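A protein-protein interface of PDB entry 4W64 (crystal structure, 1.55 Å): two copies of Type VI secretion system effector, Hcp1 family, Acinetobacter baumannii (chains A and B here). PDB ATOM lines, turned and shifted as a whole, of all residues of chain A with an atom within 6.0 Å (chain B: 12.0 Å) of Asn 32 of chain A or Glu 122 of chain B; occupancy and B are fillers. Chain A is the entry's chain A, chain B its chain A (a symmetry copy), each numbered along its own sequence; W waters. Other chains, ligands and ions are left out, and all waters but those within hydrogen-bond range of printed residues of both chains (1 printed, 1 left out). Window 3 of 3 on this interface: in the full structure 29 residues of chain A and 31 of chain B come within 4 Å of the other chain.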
ATOM      1  N   LYS A   4       5.265  25.507 -12.141  1.00  0.00           N
ATOM      2  CA  LYS A   4       6.443  26.075 -11.498  1.00  0.00           C
ATOM      3  C   LYS A   4       7.470  25.020 -11.137  1.00  0.00           C
ATOM      4  O   LYS A   4       7.144  23.988 -10.545  1.00  0.00           O
ATOM      5  CB  LYS A   4       6.038  26.830 -10.236  1.00  0.00           C
ATOM      6  CG  LYS A   4       5.141  28.021 -10.506  1.00  0.00           C
ATOM      7  CD  LYS A   4       4.442  28.461  -9.238  1.00  0.00           C
ATOM      8  CE  LYS A   4       3.771  29.814  -9.412  1.00  0.00           C
ATOM      9  NZ  LYS A   4       2.754  30.055  -8.355  1.00  0.00           N
ATOM     10  N   ILE A   6      12.069  24.942 -10.472  1.00  0.00           N
ATOM     11  CA  ILE A   6      13.389  25.552 -10.570  1.00  0.00           C
ATOM     12  C   ILE A   6      14.415  24.429 -10.482  1.00  0.00           C
ATOM     13  O   ILE A   6      14.304  23.549  -9.622  1.00  0.00           O
ATOM     14  CB  ILE A   6      13.645  26.551  -9.422  1.00  0.00           C
ATOM     15  CG1 ILE A   6      12.488  27.525  -9.257  1.00  0.00           C
ATOM     16  CG2 ILE A   6      14.951  27.305  -9.648  1.00  0.00           C
ATOM     17  CD1 ILE A   6      12.617  28.412  -8.018  1.00  0.00           C
ATOM     18  N   GLU A  30      16.392  19.852  -7.807  1.00  0.00           N
ATOM     19  CA  GLU A  30      15.129  20.587  -7.811  1.00  0.00           C
ATOM     20  C   GLU A  30      15.087  21.488  -6.589  1.00  0.00           C
ATOM     21  O   GLU A  30      15.284  21.035  -5.450  1.00  0.00           O
ATOM     22  CB  GLU A  30      13.935  19.623  -7.798  1.00  0.00           C
ATOM     23  CG  GLU A  30      13.900  18.762  -9.069  1.00  0.00           C
ATOM     24  CD  GLU A  30      12.662  17.903  -9.214  1.00  0.00           C
ATOM     25  OE1 GLU A  30      11.825  17.855  -8.285  1.00  0.00           O
ATOM     26  OE2 GLU A  30      12.529  17.267 -10.284  1.00  0.00           O
ATOM     27  N   VAL A  31      14.819  22.767  -6.823  1.00  0.00           N
ATOM     28  CA  VAL A  31      14.688  23.710  -5.720  1.00  0.00           C
ATOM     29  C   VAL A  31      13.319  24.414  -5.721  1.00  0.00           C
ATOM     30  O   VAL A  31      12.586  24.397  -6.726  1.00  0.00           O
ATOM     31  CB  VAL A  31      15.866  24.707  -5.659  1.00  0.00           C
ATOM     32  CG1 VAL A  31      17.207  23.986  -5.781  1.00  0.00           C
ATOM     33  CG2 VAL A  31      15.741  25.726  -6.733  1.00  0.00           C
ATOM     34  N   ASN A  32      12.974  25.019  -4.593  1.00  0.00           N
ATOM     35  CA  ASN A  32      11.623  25.503  -4.355  1.00  0.00           C
ATOM     36  C   ASN A  32      11.467  27.017  -4.501  1.00  0.00           C
ATOM     37  O   ASN A  32      10.376  27.505  -4.789  1.00  0.00           O
ATOM     38  CB  ASN A  32      11.184  25.124  -2.942  1.00  0.00           C
ATOM     39  CG  ASN A  32      11.297  23.638  -2.665  1.00  0.00           C
ATOM     40  OD1 ASN A  32      11.259  22.810  -3.579  1.00  0.00           O
ATOM     41  ND2 ASN A  32      11.424  23.290  -1.385  1.00  0.00           N
ATOM     42  N   SER A  33      12.545  27.754  -4.246  1.00  0.00           N
ATOM     43  CA  SER A  33      12.469  29.218  -4.232  1.00  0.00           C
ATOM     44  C   SER A  33      13.845  29.831  -4.373  1.00  0.00           C
ATOM     45  O   SER A  33      14.864  29.146  -4.214  1.00  0.00           O
ATOM     46  CB  SER A  33      11.790  29.727  -2.959  1.00  0.00           C
ATOM     47  OG  SER A  33      12.548  29.409  -1.790  1.00  0.00           O
ATOM     48  N   TRP A  34      13.864  31.129  -4.678  1.00  0.00           N
ATOM     49  CA  TRP A  34      15.112  31.852  -4.928  1.00  0.00           C
ATOM     50  C   TRP A  34      14.939  33.291  -4.490  1.00  0.00           C
ATOM     51  O   TRP A  34      13.867  33.880  -4.635  1.00  0.00           O
ATOM     52  CB  TRP A  34      15.436  31.816  -6.419  1.00  0.00           C
ATOM     53  CG  TRP A  34      16.499  32.792  -6.921  1.00  0.00           C
ATOM     54  CD1 TRP A  34      17.859  32.663  -6.818  1.00  0.00           C
ATOM     55  CD2 TRP A  34      16.264  33.984  -7.672  1.00  0.00           C
ATOM     56  NE1 TRP A  34      18.482  33.734  -7.437  1.00  0.00           N
ATOM     57  CE2 TRP A  34      17.525  34.552  -7.978  1.00  0.00           C
ATOM     58  CE3 TRP A  34      15.109  34.637  -8.113  1.00  0.00           C
ATOM     59  CZ2 TRP A  34      17.652  35.730  -8.712  1.00  0.00           C
ATOM     60  CZ3 TRP A  34      15.236  35.807  -8.837  1.00  0.00           C
ATOM     61  CH2 TRP A  34      16.501  36.346  -9.127  1.00  0.00           C
ATOM     62  N   VAL A  65      16.033  27.677  -1.626  1.00  0.00           N
ATOM     63  CA  VAL A  65      15.514  26.731  -0.646  1.00  0.00           C
ATOM     64  C   VAL A  65      15.146  25.443  -1.382  1.00  0.00           C
ATOM     65  O   VAL A  65      14.560  25.484  -2.465  1.00  0.00           O
ATOM     66  CB  VAL A  65      14.307  27.313   0.115  1.00  0.00           C
ATOM     67  CG1 VAL A  65      13.680  26.246   1.016  1.00  0.00           C
ATOM     68  CG2 VAL A  65      14.734  28.519   0.941  1.00  0.00           C
ATOM     69  N   LYS A  66      15.515  24.301  -0.806  1.00  0.00           N
ATOM     70  CA  LYS A  66      15.247  23.002  -1.432  1.00  0.00           C
ATOM     71  C   LYS A  66      14.865  21.969  -0.377  1.00  0.00           C
ATOM     72  O   LYS A  66      15.169  22.137   0.808  1.00  0.00           O
ATOM     73  CB  LYS A  66      16.482  22.513  -2.207  1.00  0.00           C
ATOM     74  CG  LYS A  66      17.719  22.297  -1.326  1.00  0.00           C
ATOM     75  CD  LYS A  66      18.906  21.736  -2.121  1.00  0.00           C
ATOM     76  CE  LYS A  66      18.725  20.262  -2.436  1.00  0.00           C
ATOM     77  NZ  LYS A  66      18.785  19.415  -1.188  1.00  0.00           N
ATOM     78  N   ASP A  67      14.186  20.902  -0.788  1.00  0.00           N
ATOM     79  CA  ASP A  67      13.982  19.784   0.144  1.00  0.00           C
ATOM     80  C   ASP A  67      15.320  19.112   0.468  1.00  0.00           C
ATOM     81  O   ASP A  67      16.200  19.008  -0.403  1.00  0.00           O
ATOM     82  CB  ASP A  67      13.030  18.731  -0.440  1.00  0.00           C
ATOM     83  CG  ASP A  67      11.654  19.291  -0.773  1.00  0.00           C
ATOM     84  OD1 ASP A  67      11.324  20.417  -0.357  1.00  0.00           O
ATOM     85  OD2 ASP A  67      10.882  18.580  -1.466  1.00  0.00           O
ATOM     86  N   THR A 127      13.702  20.816   4.823  1.00  0.00           N
ATOM     87  CA  THR A 127      14.275  21.662   3.790  1.00  0.00           C
ATOM     88  C   THR A 127      15.562  22.311   4.263  1.00  0.00           C
ATOM     89  O   THR A 127      15.900  22.300   5.453  1.00  0.00           O
ATOM     90  CB  THR A 127      13.302  22.775   3.367  1.00  0.00           C
ATOM     91  OG1 THR A 127      12.982  23.586   4.505  1.00  0.00           O
ATOM     92  CG2 THR A 127      12.016  22.206   2.778  1.00  0.00           C
ATOM     93  N   LEU B  68       8.371  40.352 -11.715  1.00  0.00           N
ATOM     94  CA  LEU B  68       9.533  40.022 -12.540  1.00  0.00           C
ATOM     95  C   LEU B  68       9.063  39.922 -13.981  1.00  0.00           C
ATOM     96  O   LEU B  68       7.993  39.365 -14.263  1.00  0.00           O
ATOM     97  CB  LEU B  68      10.156  38.691 -12.138  1.00  0.00           C
ATOM     98  CG  LEU B  68      10.840  38.555 -10.788  1.00  0.00           C
ATOM     99  CD1 LEU B  68      11.724  37.309 -10.803  1.00  0.00           C
ATOM    100  CD2 LEU B  68      11.660  39.787 -10.447  1.00  0.00           C
ATOM    101  N   PRO B 118      14.993  40.851  -6.152  1.00  0.00           N
ATOM    102  CA  PRO B 118      14.047  39.907  -6.760  1.00  0.00           C
ATOM    103  C   PRO B 118      13.843  38.632  -5.944  1.00  0.00           C
ATOM    104  O   PRO B 118      14.765  38.138  -5.262  1.00  0.00           O
ATOM    105  CB  PRO B 118      14.706  39.585  -8.111  1.00  0.00           C
ATOM    106  CG  PRO B 118      16.191  39.659  -7.814  1.00  0.00           C
ATOM    107  CD  PRO B 118      16.341  40.752  -6.764  1.00  0.00           C
ATOM    108  N   THR B 119      12.624  38.096  -6.000  1.00  0.00           N
ATOM    109  CA  THR B 119      12.314  36.823  -5.355  1.00  0.00           C
ATOM    110  C   THR B 119      11.397  35.986  -6.238  1.00  0.00           C
ATOM    111  O   THR B 119      10.516  36.520  -6.926  1.00  0.00           O
ATOM    112  CB  THR B 119      11.639  37.006  -3.974  1.00  0.00           C
ATOM    113  OG1 THR B 119      10.445  37.784  -4.112  1.00  0.00           O
ATOM    114  CG2 THR B 119      12.570  37.688  -2.981  1.00  0.00           C
ATOM    115  N   VAL B 120      11.622  34.675  -6.218  1.00  0.00           N
ATOM    116  CA  VAL B 120      10.700  33.694  -6.771  1.00  0.00           C
ATOM    117  C   VAL B 120      10.321  32.753  -5.665  1.00  0.00           C
ATOM    118  O   VAL B 120      11.163  32.022  -5.137  1.00  0.00           O
ATOM    119  CB  VAL B 120      11.346  32.907  -7.928  1.00  0.00           C
ATOM    120  CG1 VAL B 120      10.430  31.784  -8.378  1.00  0.00           C
ATOM    121  CG2 VAL B 120      11.660  33.859  -9.085  1.00  0.00           C
ATOM    122  N   ASN B 121       9.047  32.759  -5.298  1.00  0.00           N
ATOM    123  CA  ASN B 121       8.573  31.855  -4.252  1.00  0.00           C
ATOM    124  C   ASN B 121       7.860  30.647  -4.843  1.00  0.00           C
ATOM    125  O   ASN B 121       7.635  30.592  -6.053  1.00  0.00           O
ATOM    126  CB  ASN B 121       7.640  32.603  -3.300  1.00  0.00           C
ATOM    127  CG  ASN B 121       8.327  33.767  -2.607  1.00  0.00           C
ATOM    128  OD1 ASN B 121       9.459  33.643  -2.138  1.00  0.00           O
ATOM    129  ND2 ASN B 121       7.645  34.906  -2.539  1.00  0.00           N
ATOM    130  N   GLU B 122       7.521  29.669  -3.994  1.00  0.00           N
ATOM    131  CA  GLU B 122       6.770  28.506  -4.452  1.00  0.00           C
ATOM    132  C   GLU B 122       5.408  28.938  -4.959  1.00  0.00           C
ATOM    133  O   GLU B 122       4.931  28.439  -5.978  1.00  0.00           O
ATOM    134  CB  GLU B 122       6.587  27.485  -3.329  1.00  0.00           C
ATOM    135  CG  GLU B 122       7.829  26.685  -3.006  1.00  0.00           C
ATOM    136  CD  GLU B 122       7.511  25.424  -2.234  1.00  0.00           C
ATOM    137  OE1 GLU B 122       7.609  25.450  -0.989  1.00  0.00           O
ATOM    138  OE2 GLU B 122       7.168  24.406  -2.873  1.00  0.00           O
ATOM    139  N   GLU B 123       4.797  29.872  -4.239  1.00  0.00           N
ATOM    140  CA  GLU B 123       3.472  30.368  -4.573  1.00  0.00           C
ATOM    141  C   GLU B 123       3.511  31.861  -4.854  1.00  0.00           C
ATOM    142  O   GLU B 123       4.292  32.603  -4.249  1.00  0.00           O
ATOM    143  CB  GLU B 123       2.509  30.089  -3.421  1.00  0.00           C
ATOM    144  CG  GLU B 123       2.300  28.615  -3.142  1.00  0.00           C
ATOM    145  CD  GLU B 123       0.880  28.182  -3.416  1.00  0.00           C
ATOM    146  OE1 GLU B 123      -0.033  29.024  -3.277  1.00  0.00           O
ATOM    147  OE2 GLU B 123       0.676  27.003  -3.773  1.00  0.00           O
ATOM    148  N   GLY B 124       2.664  32.297  -5.777  1.00  0.00           N
ATOM    149  CA  GLY B 124       2.570  33.705  -6.100  1.00  0.00           C
ATOM    150  C   GLY B 124       3.444  34.111  -7.265  1.00  0.00           C
ATOM    151  O   GLY B 124       4.449  33.460  -7.577  1.00  0.00           O
ATOM    152  N   VAL B 125       3.044  35.196  -7.921  1.00  0.00           N
ATOM    153  CA  VAL B 125       3.790  35.765  -9.033  1.00  0.00           C
ATOM    154  C   VAL B 125       5.102  36.337  -8.513  1.00  0.00           C
ATOM    155  O   VAL B 125       5.094  37.106  -7.540  1.00  0.00           O
ATOM    156  CB  VAL B 125       2.962  36.892  -9.683  1.00  0.00           C
ATOM    157  CG1 VAL B 125       3.760  37.623 -10.744  1.00  0.00           C
ATOM    158  CG2 VAL B 125       1.683  36.323 -10.276  1.00  0.00           C
ATOM    159  N   PRO B 126       6.238  35.956  -9.133  1.00  0.00           N
ATOM    160  CA  PRO B 126       7.520  36.522  -8.708  1.00  0.00           C
ATOM    161  C   PRO B 126       7.558  38.039  -8.852  1.00  0.00           C
ATOM    162  O   PRO B 126       7.034  38.600  -9.822  1.00  0.00           O
ATOM    163  CB  PRO B 126       8.522  35.874  -9.663  1.00  0.00           C
ATOM    164  CG  PRO B 126       7.881  34.556 -10.031  1.00  0.00           C
ATOM    165  CD  PRO B 126       6.412  34.901 -10.150  1.00  0.00           C
ATOM    166  N   THR B 127       8.157  38.700  -7.869  1.00  0.00           N
ATOM    167  CA  THR B 127       8.256  40.150  -7.867  1.00  0.00           C
ATOM    168  C   THR B 127       9.639  40.606  -7.444  1.00  0.00           C
ATOM    169  O   THR B 127      10.454  39.830  -6.931  1.00  0.00           O
ATOM    170  CB  THR B 127       7.228  40.786  -6.918  1.00  0.00           C
ATOM    171  OG1 THR B 127       7.450  40.307  -5.586  1.00  0.00           O
ATOM    172  CG2 THR B 127       5.798  40.464  -7.337  1.00  0.00           C
HETATM  173  O   HOH W   1      10.389  25.376   0.436  1.00  0.00           O
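O of Trp 34 of chain A sits at hydrogen-bond distance from N of Val 120 of chain B (2.9 Å).
The side-chain amino group of Lys 4 of chain A sits close to the backbone NH of Gly 124 of chain B.
The backbone NH (N) of Asn 32 of chain A lies within hydrogen-bond range of the backbone carbonyl oxygen (O) of Val 65 of chain A (2.7 Å).
The side-chain carboxylate (OD1) of Asp 67 of chain A sits at hydrogen-bond distance from the side-chain amide nitrogen (ND2) of Asn 32 of chain A (3.1 Å).
O of Ser 33 of chain A is in hydrogen-bond range of N of Val 65 of chain A, at 3.2 Å.
The backbone NH of Thr 119 of chain B lies within hydrogen-bond range of the backbone carbonyl oxygen of Thr 127 of chain B (2.9 Å).
Among the printed residues, pairs that only touch across the chains: Asn 32 of chain A with Glu 122 of chain B, Ser 33 of chain A with Val 120 of chain B, Lys 4 of chain A with Glu 122 of chain B, Trp 34 of chain A with Thr 119 of chain B, Trp 34 of chain A with Pro 118 of chain B and Lys 4 of chain A with Glu 123 of chain B.
Printed residues of chain B within 4 Å of Asn 32 of chain A: Glu 122.
Of the printed residues of chain A, Glu 122 of chain B touches Lys 4 and Asn 32.
Ile 6 of chain A touches none of the printed residues of chain B.
Val 65 of chain A touches none of the printed residues of chain B.
Asp 67 of chain A touches none of the printed residues of chain B.
Of the printed residues of chain B, Ser 33 of chain A touches Val 120 (3.2 Å).
Of the printed residues of chain A, Thr 119 of chain B touches Trp 34.
Of the printed residues of chain B, Lys 4 of chain A touches Glu 122, Glu 123 and Gly 124.
Of the printed residues of chain A, Glu 123 of chain B touches Lys 4.
Leu 68 of chain B touches none of the printed residues of chain A.
Pro 126 of chain B touches none of the printed residues of chain A.
The nearest printed residue of chain B that does not touch Asn 32 of chain A is Asn 121 of chain B (4.03 Å).
Of the 11 printed residues of chain A, 4 touch a printed residue of chain B.
Hydrophobic or aromatic side chains of chain A within 4 Å of the printed part of chain B: Trp 34.
Of the 11 printed residues of chain B, 6 touch a printed residue of chain A.
1 position is printed for both chains.
Of the 8 pairs that touch across the chains among the printed residues, none has its exchanged pair printed and touching as well.
Water W1 bridges ND2 of Asn 32 of chain A and OE1 of Glu 122 of chain B.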
